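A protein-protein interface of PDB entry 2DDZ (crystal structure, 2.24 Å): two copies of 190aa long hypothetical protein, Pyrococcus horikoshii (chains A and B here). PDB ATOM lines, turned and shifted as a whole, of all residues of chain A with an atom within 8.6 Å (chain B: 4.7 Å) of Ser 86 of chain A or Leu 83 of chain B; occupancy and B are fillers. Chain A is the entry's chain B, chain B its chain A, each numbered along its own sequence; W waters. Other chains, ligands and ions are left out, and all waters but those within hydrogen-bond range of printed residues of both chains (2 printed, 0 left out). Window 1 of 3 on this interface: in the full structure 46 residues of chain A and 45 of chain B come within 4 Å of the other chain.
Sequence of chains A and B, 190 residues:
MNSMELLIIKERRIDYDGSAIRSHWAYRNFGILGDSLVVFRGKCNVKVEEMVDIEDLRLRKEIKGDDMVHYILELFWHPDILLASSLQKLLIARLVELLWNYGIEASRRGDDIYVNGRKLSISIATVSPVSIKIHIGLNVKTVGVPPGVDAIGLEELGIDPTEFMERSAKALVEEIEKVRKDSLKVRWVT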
ATOM      1  N   TRP A  77     -29.402  -0.843 -25.637  1.00  0.00           N
ATOM      2  CA  TRP A  77     -28.577  -0.560 -24.456  1.00  0.00           C
ATOM      3  C   TRP A  77     -27.171  -0.689 -25.011  1.00  0.00           C
ATOM      4  O   TRP A  77     -27.010  -0.968 -26.196  1.00  0.00           O
ATOM      5  CB  TRP A  77     -28.801  -1.616 -23.379  1.00  0.00           C
ATOM      6  CG  TRP A  77     -30.228  -1.703 -22.944  1.00  0.00           C
ATOM      7  CD1 TRP A  77     -31.233  -0.847 -23.287  1.00  0.00           C
ATOM      8  CD2 TRP A  77     -30.780  -2.598 -21.966  1.00  0.00           C
ATOM      9  NE1 TRP A  77     -32.373  -1.146 -22.587  1.00  0.00           N
ATOM     10  CE2 TRP A  77     -32.134  -2.226 -21.776  1.00  0.00           C
ATOM     11  CE3 TRP A  77     -30.277  -3.692 -21.258  1.00  0.00           C
ATOM     12  CZ2 TRP A  77     -32.975  -2.878 -20.865  1.00  0.00           C
ATOM     13  CZ3 TRP A  77     -31.118  -4.350 -20.352  1.00  0.00           C
ATOM     14  CH2 TRP A  77     -32.457  -3.948 -20.179  1.00  0.00           C
ATOM     15  N   HIS A  78     -26.158  -0.492 -24.176  1.00  0.00           N
ATOM     16  CA  HIS A  78     -24.784  -0.623 -24.630  1.00  0.00           C
ATOM     17  C   HIS A  78     -24.621  -2.022 -25.201  1.00  0.00           C
ATOM     18  O   HIS A  78     -24.912  -2.999 -24.520  1.00  0.00           O
ATOM     19  CB  HIS A  78     -23.793  -0.457 -23.478  1.00  0.00           C
ATOM     20  CG  HIS A  78     -22.367  -0.404 -23.927  1.00  0.00           C
ATOM     21  ND1 HIS A  78     -21.311  -0.735 -23.107  1.00  0.00           N
ATOM     22  CD2 HIS A  78     -21.823  -0.048 -25.117  1.00  0.00           C
ATOM     23  CE1 HIS A  78     -20.178  -0.585 -23.772  1.00  0.00           C
ATOM     24  NE2 HIS A  78     -20.461  -0.168 -24.992  1.00  0.00           N
ATOM     25  N   ASP A  80     -23.148  -4.746 -25.270  1.00  0.00           N
ATOM     26  CA  ASP A  80     -22.181  -5.560 -24.541  1.00  0.00           C
ATOM     27  C   ASP A  80     -22.587  -7.039 -24.578  1.00  0.00           C
ATOM     28  O   ASP A  80     -23.695  -7.401 -24.180  1.00  0.00           O
ATOM     29  CB  ASP A  80     -22.100  -5.070 -23.089  1.00  0.00           C
ATOM     30  CG  ASP A  80     -20.966  -5.720 -22.304  1.00  0.00           C
ATOM     31  OD1 ASP A  80     -20.704  -6.927 -22.500  1.00  0.00           O
ATOM     32  OD2 ASP A  80     -20.345  -5.022 -21.475  1.00  0.00           O
ATOM     33  N   ILE A  81     -21.691  -7.892 -25.058  1.00  0.00           N
ATOM     34  CA  ILE A  81     -21.977  -9.317 -25.114  1.00  0.00           C
ATOM     35  C   ILE A  81     -22.247  -9.930 -23.730  1.00  0.00           C
ATOM     36  O   ILE A  81     -23.044 -10.866 -23.606  1.00  0.00           O
ATOM     37  CB  ILE A  81     -20.817 -10.109 -25.780  1.00  0.00           C
ATOM     38  CG1 ILE A  81     -19.499  -9.829 -25.044  1.00  0.00           C
ATOM     39  CG2 ILE A  81     -20.708  -9.737 -27.251  1.00  0.00           C
ATOM     40  CD1 ILE A  81     -18.291 -10.671 -25.535  1.00  0.00           C
ATOM     41  N   LEU A  82     -21.580  -9.434 -22.689  1.00  0.00           N
ATOM     42  CA  LEU A  82     -21.807  -9.982 -21.350  1.00  0.00           C
ATOM     43  C   LEU A  82     -23.242  -9.672 -20.900  1.00  0.00           C
ATOM     44  O   LEU A  82     -23.913 -10.500 -20.277  1.00  0.00           O
ATOM     45  CB  LEU A  82     -20.793  -9.405 -20.355  1.00  0.00           C
ATOM     46  CG  LEU A  82     -19.436 -10.113 -20.376  1.00  0.00           C
ATOM     47  CD1 LEU A  82     -18.395  -9.304 -19.619  1.00  0.00           C
ATOM     48  CD2 LEU A  82     -19.591 -11.505 -19.777  1.00  0.00           C
ATOM     49  N   LEU A  83     -23.714  -8.481 -21.246  1.00  0.00           N
ATOM     50  CA  LEU A  83     -25.065  -8.073 -20.896  1.00  0.00           C
ATOM     51  C   LEU A  83     -26.092  -8.868 -21.697  1.00  0.00           C
ATOM     52  O   LEU A  83     -27.131  -9.275 -21.174  1.00  0.00           O
ATOM     53  CB  LEU A  83     -25.242  -6.580 -21.166  1.00  0.00           C
ATOM     54  CG  LEU A  83     -26.650  -6.010 -20.965  1.00  0.00           C
ATOM     55  CD1 LEU A  83     -27.200  -6.446 -19.619  1.00  0.00           C
ATOM     56  CD2 LEU A  83     -26.601  -4.502 -21.069  1.00  0.00           C
ATOM     57  N   ALA A  84     -25.801  -9.095 -22.969  1.00  0.00           N
ATOM     58  CA  ALA A  84     -26.725  -9.847 -23.809  1.00  0.00           C
ATOM     59  C   ALA A  84     -26.818 -11.262 -23.265  1.00  0.00           C
ATOM     60  O   ALA A  84     -27.902 -11.847 -23.188  1.00  0.00           O
ATOM     61  CB  ALA A  84     -26.235  -9.863 -25.276  1.00  0.00           C
ATOM     62  N   SER A  85     -25.672 -11.806 -22.869  1.00  0.00           N
ATOM     63  CA  SER A  85     -25.638 -13.162 -22.342  1.00  0.00           C
ATOM     64  C   SER A  85     -26.353 -13.312 -20.991  1.00  0.00           C
ATOM     65  O   SER A  85     -27.100 -14.252 -20.800  1.00  0.00           O
ATOM     66  CB  SER A  85     -24.190 -13.647 -22.229  1.00  0.00           C
ATOM     67  OG  SER A  85     -24.159 -14.962 -21.703  1.00  0.00           O
ATOM     68  N   SER A  86     -26.124 -12.398 -20.060  1.00  0.00           N
ATOM     69  CA  SER A  86     -26.774 -12.503 -18.762  1.00  0.00           C
ATOM     70  C   SER A  86     -28.293 -12.275 -18.862  1.00  0.00           C
ATOM     71  O   SER A  86     -29.094 -13.023 -18.296  1.00  0.00           O
ATOM     72  CB  SER A  86     -26.144 -11.504 -17.783  1.00  0.00           C
ATOM     73  OG  SER A  86     -26.185 -10.205 -18.325  1.00  0.00           O
ATOM     74  N   LEU A  87     -28.683 -11.237 -19.594  1.00  0.00           N
ATOM     75  CA  LEU A  87     -30.092 -10.911 -19.758  1.00  0.00           C
ATOM     76  C   LEU A  87     -30.815 -12.087 -20.407  1.00  0.00           C
ATOM     77  O   LEU A  87     -31.957 -12.420 -20.067  1.00  0.00           O
ATOM     78  CB  LEU A  87     -30.234  -9.658 -20.622  1.00  0.00           C
ATOM     79  CG  LEU A  87     -31.614  -9.006 -20.681  1.00  0.00           C
ATOM     80  CD1 LEU A  87     -32.114  -8.660 -19.289  1.00  0.00           C
ATOM     81  CD2 LEU A  87     -31.498  -7.770 -21.513  1.00  0.00           C
ATOM     82  N   GLN A  88     -30.134 -12.722 -21.343  1.00  0.00           N
ATOM     83  CA  GLN A  88     -30.695 -13.879 -22.020  1.00  0.00           C
ATOM     84  C   GLN A  88     -31.041 -14.948 -21.027  1.00  0.00           C
ATOM     85  O   GLN A  88     -32.172 -15.421 -20.974  1.00  0.00           O
ATOM     86  CB  GLN A  88     -29.691 -14.500 -22.996  1.00  0.00           C
ATOM     87  CG  GLN A  88     -30.048 -15.944 -23.371  1.00  0.00           C
ATOM     88  CD  GLN A  88     -28.934 -16.652 -24.133  1.00  0.00           C
ATOM     89  OE1 GLN A  88     -27.768 -16.602 -23.738  1.00  0.00           O
ATOM     90  NE2 GLN A  88     -29.293 -17.326 -25.223  1.00  0.00           N
ATOM     91  N   LYS A  89     -30.046 -15.356 -20.253  1.00  0.00           N
ATOM     92  CA  LYS A  89     -30.286 -16.416 -19.309  1.00  0.00           C
ATOM     93  C   LYS A  89     -31.317 -16.069 -18.230  1.00  0.00           C
ATOM     94  O   LYS A  89     -32.028 -16.948 -17.771  1.00  0.00           O
ATOM     95  CB  LYS A  89     -28.951 -16.920 -18.760  1.00  0.00           C
ATOM     96  CG  LYS A  89     -28.340 -17.960 -19.724  1.00  0.00           C
ATOM     97  CD  LYS A  89     -26.863 -18.231 -19.509  1.00  0.00           C
ATOM     98  CE  LYS A  89     -26.011 -17.150 -20.151  1.00  0.00           C
ATOM     99  NZ  LYS A  89     -26.092 -17.214 -21.636  1.00  0.00           N
ATOM    100  N   LEU A  90     -31.437 -14.797 -17.862  1.00  0.00           N
ATOM    101  CA  LEU A  90     -32.444 -14.407 -16.872  1.00  0.00           C
ATOM    102  C   LEU A  90     -33.829 -14.628 -17.506  1.00  0.00           C
ATOM    103  O   LEU A  90     -34.754 -15.114 -16.844  1.00  0.00           O
ATOM    104  CB  LEU A  90     -32.289 -12.932 -16.481  1.00  0.00           C
ATOM    105  CG  LEU A  90     -33.441 -12.331 -15.656  1.00  0.00           C
ATOM    106  CD1 LEU A  90     -33.507 -12.983 -14.279  1.00  0.00           C
ATOM    107  CD2 LEU A  90     -33.228 -10.844 -15.501  1.00  0.00           C
ATOM    108  N   LEU A  91     -33.964 -14.289 -18.794  1.00  0.00           N
ATOM    109  CA  LEU A  91     -35.237 -14.470 -19.486  1.00  0.00           C
ATOM    110  C   LEU A  91     -35.604 -15.954 -19.570  1.00  0.00           C
ATOM    111  O   LEU A  91     -36.738 -16.328 -19.255  1.00  0.00           O
ATOM    112  CB  LEU A  91     -35.194 -13.830 -20.892  1.00  0.00           C
ATOM    113  CG  LEU A  91     -35.066 -12.296 -20.892  1.00  0.00           C
ATOM    114  CD1 LEU A  91     -34.898 -11.787 -22.297  1.00  0.00           C
ATOM    115  CD2 LEU A  91     -36.286 -11.664 -20.242  1.00  0.00           C
ATOM    116  N   ILE A  92     -34.660 -16.796 -19.996  1.00  0.00           N
ATOM    117  CA  ILE A  92     -34.904 -18.236 -20.066  1.00  0.00           C
ATOM    118  C   ILE A  92     -35.357 -18.699 -18.679  1.00  0.00           C
ATOM    119  O   ILE A  92     -36.274 -19.505 -18.554  1.00  0.00           O
ATOM    120  CB  ILE A  92     -33.619 -19.007 -20.436  1.00  0.00           C
ATOM    121  CG1 ILE A  92     -33.234 -18.678 -21.880  1.00  0.00           C
ATOM    122  CG2 ILE A  92     -33.834 -20.522 -20.326  1.00  0.00           C
ATOM    123  CD1 ILE A  92     -34.269 -19.116 -22.892  1.00  0.00           C
ATOM    124  N   ALA A  93     -34.713 -18.171 -17.639  1.00  0.00           N
ATOM    125  CA  ALA A  93     -35.044 -18.532 -16.267  1.00  0.00           C
ATOM    126  C   ALA A  93     -36.462 -18.093 -15.905  1.00  0.00           C
ATOM    127  O   ALA A  93     -37.165 -18.797 -15.184  1.00  0.00           O
ATOM    128  CB  ALA A  93     -34.030 -17.906 -15.297  1.00  0.00           C
ATOM    129  N   ARG A 108     -33.608 -25.522 -15.862  1.00  0.00           N
ATOM    130  CA  ARG A 108     -32.755 -24.778 -16.770  1.00  0.00           C
ATOM    131  C   ARG A 108     -31.339 -25.349 -16.798  1.00  0.00           C
ATOM    132  O   ARG A 108     -30.845 -25.854 -15.789  1.00  0.00           O
ATOM    133  CB  ARG A 108     -32.692 -23.305 -16.355  1.00  0.00           C
ATOM    134  CG  ARG A 108     -31.792 -22.460 -17.258  1.00  0.00           C
ATOM    135  CD  ARG A 108     -31.958 -20.980 -16.992  1.00  0.00           C
ATOM    136  NE  ARG A 108     -31.571 -20.609 -15.632  1.00  0.00           N
ATOM    137  CZ  ARG A 108     -30.344 -20.244 -15.268  1.00  0.00           C
ATOM    138  NH1 ARG A 108     -29.362 -20.198 -16.166  1.00  0.00           N
ATOM    139  NH2 ARG A 108     -30.097 -19.923 -14.004  1.00  0.00           N
ATOM    140  N   GLY A 110     -28.216 -23.583 -18.387  1.00  0.00           N
ATOM    141  CA  GLY A 110     -27.633 -22.462 -19.101  1.00  0.00           C
ATOM    142  C   GLY A 110     -28.736 -21.666 -19.778  1.00  0.00           C
ATOM    143  O   GLY A 110     -29.525 -20.967 -19.126  1.00  0.00           O
ATOM    144  N   ALA A 125     -27.973 -15.150 -27.939  1.00  0.00           N
ATOM    145  CA  ALA A 125     -27.903 -13.771 -27.514  1.00  0.00           C
ATOM    146  C   ALA A 125     -26.646 -13.208 -28.136  1.00  0.00           C
ATOM    147  O   ALA A 125     -25.585 -13.840 -28.086  1.00  0.00           O
ATOM    148  CB  ALA A 125     -27.812 -13.696 -25.981  1.00  0.00           C
ATOM    149  N   ILE A 132     -28.667  -4.833 -28.622  1.00  0.00           N
ATOM    150  CA  ILE A 132     -28.576  -6.186 -28.106  1.00  0.00           C
ATOM    151  C   ILE A 132     -29.718  -6.964 -28.755  1.00  0.00           C
ATOM    152  O   ILE A 132     -30.820  -6.445 -28.883  1.00  0.00           O
ATOM    153  CB  ILE A 132     -28.773  -6.213 -26.580  1.00  0.00           C
ATOM    154  CG1 ILE A 132     -27.514  -5.699 -25.883  1.00  0.00           C
ATOM    155  CG2 ILE A 132     -29.115  -7.629 -26.138  1.00  0.00           C
ATOM    156  CD1 ILE A 132     -27.672  -5.551 -24.384  1.00  0.00           C
ATOM    157  N   ILE A 134     -31.695 -10.863 -28.833  1.00  0.00           N
ATOM    158  CA  ILE A 134     -31.868 -12.196 -28.307  1.00  0.00           C
ATOM    159  C   ILE A 134     -33.006 -12.932 -28.985  1.00  0.00           C
ATOM    160  O   ILE A 134     -34.028 -12.341 -29.319  1.00  0.00           O
ATOM    161  CB  ILE A 134     -32.199 -12.126 -26.804  1.00  0.00           C
ATOM    162  CG1 ILE A 134     -31.008 -11.542 -26.043  1.00  0.00           C
ATOM    163  CG2 ILE A 134     -32.645 -13.495 -26.304  1.00  0.00           C
ATOM    164  CD1 ILE A 134     -31.333 -11.150 -24.627  1.00  0.00           C
ATOM    165  N   GLU A 175     -40.144  -8.599 -16.651  1.00  0.00           N
ATOM    166  CA  GLU A 175     -38.794  -8.928 -16.177  1.00  0.00           C
ATOM    167  C   GLU A 175     -37.808  -7.835 -16.570  1.00  0.00           C
ATOM    168  O   GLU A 175     -37.018  -7.354 -15.754  1.00  0.00           O
ATOM    169  CB  GLU A 175     -38.338 -10.265 -16.770  1.00  0.00           C
ATOM    170  CG  GLU A 175     -37.068 -10.837 -16.152  1.00  0.00           C
ATOM    171  CD  GLU A 175     -37.216 -11.125 -14.661  1.00  0.00           C
ATOM    172  OE1 GLU A 175     -38.198 -11.789 -14.273  1.00  0.00           O
ATOM    173  OE2 GLU A 175     -36.350 -10.689 -13.875  1.00  0.00           O
ATOM    174  N   VAL A 179     -35.657  -5.002 -14.351  1.00  0.00           N
ATOM    175  CA  VAL A 179     -34.209  -4.934 -14.482  1.00  0.00           C
ATOM    176  C   VAL A 179     -33.830  -3.460 -14.598  1.00  0.00           C
ATOM    177  O   VAL A 179     -32.918  -2.979 -13.934  1.00  0.00           O
ATOM    178  CB  VAL A 179     -33.700  -5.666 -15.738  1.00  0.00           C
ATOM    179  CG1 VAL A 179     -32.282  -5.181 -16.095  1.00  0.00           C
ATOM    180  CG2 VAL A 179     -33.670  -7.160 -15.487  1.00  0.00           C
ATOM    181  N   ARG A 180     -34.570  -2.752 -15.440  1.00  0.00           N
ATOM    182  CA  ARG A 180     -34.332  -1.340 -15.679  1.00  0.00           C
ATOM    183  C   ARG A 180     -34.567  -0.477 -14.422  1.00  0.00           C
ATOM    184  O   ARG A 180     -33.697   0.296 -14.025  1.00  0.00           O
ATOM    185  CB  ARG A 180     -35.221  -0.881 -16.842  1.00  0.00           C
ATOM    186  CG  ARG A 180     -34.734   0.339 -17.592  1.00  0.00           C
ATOM    187  CD  ARG A 180     -35.720   0.749 -18.680  1.00  0.00           C
ATOM    188  NE  ARG A 180     -35.575   0.002 -19.929  1.00  0.00           N
ATOM    189  CZ  ARG A 180     -36.594  -0.527 -20.605  1.00  0.00           C
ATOM    190  NH1 ARG A 180     -37.834  -0.401 -20.142  1.00  0.00           N
ATOM    191  NH2 ARG A 180     -36.382  -1.179 -21.746  1.00  0.00           N
ATOM    192  N   SER A 183     -32.080  -0.794 -11.721  1.00  0.00           N
ATOM    193  CA  SER A 183     -30.820  -0.185 -12.130  1.00  0.00           C
ATOM    194  C   SER A 183     -30.791   1.325 -11.939  1.00  0.00           C
ATOM    195  O   SER A 183     -29.720   1.934 -12.010  1.00  0.00           O
ATOM    196  CB  SER A 183     -30.517  -0.520 -13.604  1.00  0.00           C
ATOM    197  OG  SER A 183     -31.134   0.407 -14.488  1.00  0.00           O
ATOM    198  N   TRP B  77     -15.929  -5.913 -14.952  1.00  0.00           N
ATOM    199  CA  TRP B  77     -16.441  -5.841 -16.316  1.00  0.00           C
ATOM    200  C   TRP B  77     -16.842  -4.378 -16.469  1.00  0.00           C
ATOM    201  O   TRP B  77     -16.668  -3.588 -15.537  1.00  0.00           O
ATOM    202  CB  TRP B  77     -17.662  -6.755 -16.487  1.00  0.00           C
ATOM    203  CG  TRP B  77     -17.409  -8.226 -16.155  1.00  0.00           C
ATOM    204  CD1 TRP B  77     -16.211  -8.794 -15.819  1.00  0.00           C
ATOM    205  CD2 TRP B  77     -18.370  -9.310 -16.180  1.00  0.00           C
ATOM    206  NE1 TRP B  77     -16.364 -10.147 -15.630  1.00  0.00           N
ATOM    207  CE2 TRP B  77     -17.674 -10.495 -15.830  1.00  0.00           C
ATOM    208  CE3 TRP B  77     -19.747  -9.390 -16.438  1.00  0.00           C
ATOM    209  CZ2 TRP B  77     -18.299 -11.751 -15.768  1.00  0.00           C
ATOM    210  CZ3 TRP B  77     -20.377 -10.651 -16.372  1.00  0.00           C
ATOM    211  CH2 TRP B  77     -19.650 -11.808 -16.027  1.00  0.00           C
ATOM    212  N   HIS B  78     -17.365  -4.003 -17.626  1.00  0.00           N
ATOM    213  CA  HIS B  78     -17.788  -2.625 -17.823  1.00  0.00           C
ATOM    214  C   HIS B  78     -18.801  -2.261 -16.740  1.00  0.00           C
ATOM    215  O   HIS B  78     -19.846  -2.897 -16.621  1.00  0.00           O
ATOM    216  CB  HIS B  78     -18.442  -2.447 -19.193  1.00  0.00           C
ATOM    217  CG  HIS B  78     -18.642  -1.017 -19.573  1.00  0.00           C
ATOM    218  ND1 HIS B  78     -19.452  -0.627 -20.616  1.00  0.00           N
ATOM    219  CD2 HIS B  78     -18.127   0.122 -19.049  1.00  0.00           C
ATOM    220  CE1 HIS B  78     -19.430   0.691 -20.718  1.00  0.00           C
ATOM    221  NE2 HIS B  78     -18.635   1.169 -19.779  1.00  0.00           N
ATOM    222  N   ASP B  80     -21.660  -1.200 -15.792  1.00  0.00           N
ATOM    223  CA  ASP B  80     -22.943  -0.837 -16.375  1.00  0.00           C
ATOM    224  C   ASP B  80     -24.020  -1.216 -15.353  1.00  0.00           C
ATOM    225  O   ASP B  80     -24.133  -2.381 -14.984  1.00  0.00           O
ATOM    226  CB  ASP B  80     -23.122  -1.648 -17.662  1.00  0.00           C
ATOM    227  CG  ASP B  80     -24.320  -1.221 -18.480  1.00  0.00           C
ATOM    228  OD1 ASP B  80     -25.435  -1.118 -17.926  1.00  0.00           O
ATOM    229  OD2 ASP B  80     -24.141  -1.007 -19.698  1.00  0.00           O
ATOM    230  N   ILE B  81     -24.804  -0.244 -14.890  1.00  0.00           N
ATOM    231  CA  ILE B  81     -25.855  -0.538 -13.916  1.00  0.00           C
ATOM    232  C   ILE B  81     -26.846  -1.601 -14.439  1.00  0.00           C
ATOM    233  O   ILE B  81     -27.310  -2.438 -13.677  1.00  0.00           O
ATOM    234  CB  ILE B  81     -26.614   0.770 -13.464  1.00  0.00           C
ATOM    235  CG1 ILE B  81     -27.041   1.611 -14.673  1.00  0.00           C
ATOM    236  CG2 ILE B  81     -25.726   1.622 -12.553  1.00  0.00           C
ATOM    237  CD1 ILE B  81     -28.274   1.109 -15.361  1.00  0.00           C
ATOM    238  N   LEU B  82     -27.150  -1.595 -15.737  1.00  0.00           N
ATOM    239  CA  LEU B  82     -28.065  -2.590 -16.302  1.00  0.00           C
ATOM    240  C   LEU B  82     -27.495  -3.997 -16.215  1.00  0.00           C
ATOM    241  O   LEU B  82     -28.208  -4.959 -15.913  1.00  0.00           O
ATOM    242  CB  LEU B  82     -28.391  -2.247 -17.763  1.00  0.00           C
ATOM    243  CG  LEU B  82     -29.332  -1.043 -17.875  1.00  0.00           C
ATOM    244  CD1 LEU B  82     -29.400  -0.549 -19.313  1.00  0.00           C
ATOM    245  CD2 LEU B  82     -30.721  -1.446 -17.352  1.00  0.00           C
ATOM    246  N   LEU B  83     -26.204  -4.119 -16.492  1.00  0.00           N
ATOM    247  CA  LEU B  83     -25.545  -5.413 -16.410  1.00  0.00           C
ATOM    248  C   LEU B  83     -25.561  -5.883 -14.951  1.00  0.00           C
ATOM    249  O   LEU B  83     -25.803  -7.054 -14.663  1.00  0.00           O
ATOM    250  CB  LEU B  83     -24.093  -5.300 -16.901  1.00  0.00           C
ATOM    251  CG  LEU B  83     -23.253  -6.557 -16.700  1.00  0.00           C
ATOM    252  CD1 LEU B  83     -23.982  -7.733 -17.318  1.00  0.00           C
ATOM    253  CD2 LEU B  83     -21.860  -6.371 -17.304  1.00  0.00           C
ATOM    254  N   ALA B  84     -25.297  -4.970 -14.026  1.00  0.00           N
ATOM    255  CA  ALA B  84     -25.302  -5.342 -12.618  1.00  0.00           C
ATOM    256  C   ALA B  84     -26.684  -5.860 -12.223  1.00  0.00           C
ATOM    257  O   ALA B  84     -26.798  -6.892 -11.547  1.00  0.00           O
ATOM    258  CB  ALA B  84     -24.914  -4.140 -11.750  1.00  0.00           C
ATOM    259  N   SER B  85     -27.730  -5.150 -12.650  1.00  0.00           N
ATOM    260  CA  SER B  85     -29.116  -5.526 -12.331  1.00  0.00           C
ATOM    261  C   SER B  85     -29.560  -6.843 -12.963  1.00  0.00           C
ATOM    262  O   SER B  85     -30.256  -7.638 -12.331  1.00  0.00           O
ATOM    263  CB  SER B  85     -30.076  -4.415 -12.764  1.00  0.00           C
ATOM    264  OG  SER B  85     -31.421  -4.734 -12.440  1.00  0.00           O
ATOM    265  N   SER B  86     -29.161  -7.079 -14.207  1.00  0.00           N
ATOM    266  CA  SER B  86     -29.542  -8.306 -14.893  1.00  0.00           C
ATOM    267  C   SER B  86     -28.874  -9.496 -14.231  1.00  0.00           C
ATOM    268  O   SER B  86     -29.500 -10.527 -13.972  1.00  0.00           O
ATOM    269  CB  SER B  86     -29.126  -8.254 -16.374  1.00  0.00           C
ATOM    270  OG  SER B  86     -29.806  -7.220 -17.059  1.00  0.00           O
ATOM    271  N   LEU B  87     -27.584  -9.344 -13.971  1.00  0.00           N
ATOM    272  CA  LEU B  87     -26.802 -10.397 -13.356  1.00  0.00           C
ATOM    273  C   LEU B  87     -27.349 -10.736 -11.971  1.00  0.00           C
ATOM    274  O   LEU B  87     -27.510 -11.913 -11.619  1.00  0.00           O
ATOM    275  CB  LEU B  87     -25.348  -9.946 -13.274  1.00  0.00           C
ATOM    276  CG  LEU B  87     -24.267 -11.024 -13.269  1.00  0.00           C
ATOM    277  CD1 LEU B  87     -24.608 -12.139 -14.233  1.00  0.00           C
ATOM    278  CD2 LEU B  87     -22.960 -10.371 -13.656  1.00  0.00           C
ATOM    279  N   LEU B  90     -30.438 -12.877 -12.232  1.00  0.00           N
ATOM    280  CA  LEU B  90     -30.187 -14.208 -12.745  1.00  0.00           C
ATOM    281  C   LEU B  90     -29.693 -15.056 -11.544  1.00  0.00           C
ATOM    282  O   LEU B  90     -30.135 -16.193 -11.333  1.00  0.00           O
ATOM    283  CB  LEU B  90     -29.118 -14.150 -13.832  1.00  0.00           C
ATOM    284  CG  LEU B  90     -28.594 -15.504 -14.321  1.00  0.00           C
ATOM    285  CD1 LEU B  90     -29.716 -16.333 -14.951  1.00  0.00           C
ATOM    286  CD2 LEU B  90     -27.478 -15.244 -15.328  1.00  0.00           C
ATOM    287  N   ILE B 132     -18.481  -4.106 -11.071  1.00  0.00           N
ATOM    288  CA  ILE B 132     -19.863  -4.387 -10.730  1.00  0.00           C
ATOM    289  C   ILE B 132     -19.813  -5.020  -9.345  1.00  0.00           C
ATOM    290  O   ILE B 132     -18.950  -5.863  -9.095  1.00  0.00           O
ATOM    291  CB  ILE B 132     -20.508  -5.411 -11.693  1.00  0.00           C
ATOM    292  CG1 ILE B 132     -20.839  -4.757 -13.042  1.00  0.00           C
ATOM    293  CG2 ILE B 132     -21.774  -5.998 -11.053  1.00  0.00           C
ATOM    294  CD1 ILE B 132     -19.620  -4.378 -13.849  1.00  0.00           C
ATOM    295  N   VAL B 179     -22.164 -17.507 -18.292  1.00  0.00           N
ATOM    296  CA  VAL B 179     -22.534 -16.229 -18.857  1.00  0.00           C
ATOM    297  C   VAL B 179     -21.350 -15.729 -19.682  1.00  0.00           C
ATOM    298  O   VAL B 179     -21.503 -15.255 -20.815  1.00  0.00           O
ATOM    299  CB  VAL B 179     -22.862 -15.195 -17.763  1.00  0.00           C
ATOM    300  CG1 VAL B 179     -22.742 -13.796 -18.345  1.00  0.00           C
ATOM    301  CG2 VAL B 179     -24.294 -15.424 -17.219  1.00  0.00           C
HETATM  302  O   HOH W   1     -18.560  -5.985 -19.653  1.00  0.00           O
HETATM  303  O   HOH W   2     -26.518  -0.439 -21.142  1.00  0.00           O
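Water W1 bridges the side-chain carboxylate of Asp 80 of chain A (2.7 Å) and the backbone NH of His 78 of chain B (3.1 Å). Water W2 lies within hydrogen-bond range of the side-chain carboxylate of Asp 80 of chain B and the backbone NH of His 78 of chain A.
Printed residues of chain B within 4 Å of His 78 of chain A: His 78 (3.1 Å) and Asp 80 (3.8 Å). Of the printed residues of chain B, Leu 82 of chain A touches Trp 77 and Val 179. Of the printed residues of chain B, Leu 90 of chain A touches Leu 90. Gly 110 of chain A touches none of the printed residues of chain B. Ile 134 of chain A touches none of the printed residues of chain B. Leu 83 of chain B touches just these residues of chain A: Leu 83 and Ser 86. No residue of chain A comes within 4 Å of Ala 84 of chain B. The nearest printed residue of chain A that does not touch Trp 77 of chain B is Asp 80 of chain A (5.9 Å).
A ring nitrogen (ND1) of His 78 of chain B is in hydrogen-bond range of a ring nitrogen (ND1) of His 78 of chain A (3.1 Å). OG of Ser 85 of chain B lies within hydrogen-bond range of O of Val 179 of chain A, 2.7 Å away. OG of Ser 85 of chain A sits at hydrogen-bond distance from O of Val 179 of chain B (2.8 Å).
Of the 13 printed residues of chain B, 11 touch a printed residue of chain A. Printed residues of chain B that touch a printed residue of chain A: Trp 77, His 78, Asp 80, Ile 81, Leu 82, Leu 83, Ser 85, Ser 86, Leu 87, Leu 90 and Val 179.
The side-chain carboxylate (OD1) of Asp 80 of chain B is in hydrogen-bond range of the backbone NH (N) of Leu 82 of chain B (2.8 Å). O of Leu 82 of chain B lies within hydrogen-bond range of OG of Ser 86 of chain B, 3.0 Å away. The guanidinium group of Arg 108 of chain A is in hydrogen-bond range of the backbone carbonyl oxygen of Gly 110 of chain A (3.1 Å).
His 78 of chain B touches its own counterpart, His 78 of chain A. Leu 83 of chain A touches its own counterpart, Leu 83 of chain B. Of the 21 pairs that touch across the chains among the printed residues, 13 have their exchanged pair printed and touching as well.
Among the printed residues, pairs that only touch across the chains: Ser 183 of chain A with Ile 81 of chain B (3.1 Å), Val 179 of chain A with Ser 86 of chain B (3.3 Å), Ser 183 of chain A with Leu 82 of chain B (3.4 Å), Leu 82 of chain A with Trp 77 of chain B (3.4 Å), Ser 86 of chain A with Leu 83 of chain B (3.5 Å), Leu 87 of chain A with Ser 86 of chain B (3.5 Å), Trp 77 of chain A with Leu 82 of chain B (3.6 Å), Lys 89 of chain A with Leu 90 of chain B (3.7 Å), Leu 90 of chain A with Leu 90 of chain B (3.7 Å), Arg 108 of chain A with Leu 90 of chain B (3.7 Å), Leu 83 of chain A with Ser 86 of chain B (3.7 Å), Leu 83 of chain A with Leu 83 of chain B (3.8 Å), Lys 89 of chain A with Val 179 of chain B (3.8 Å), His 78 of chain A with Asp 80 of chain B (3.8 Å), Ser 86 of chain A with Leu 87 of chain B (3.9 Å), Asp 80 of chain A with His 78 of chain B (3.9 Å), Arg 180 of chain A with Leu 82 of chain B (3.98 Å) and Leu 82 of chain A with Val 179 of chain B (3.996 Å).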
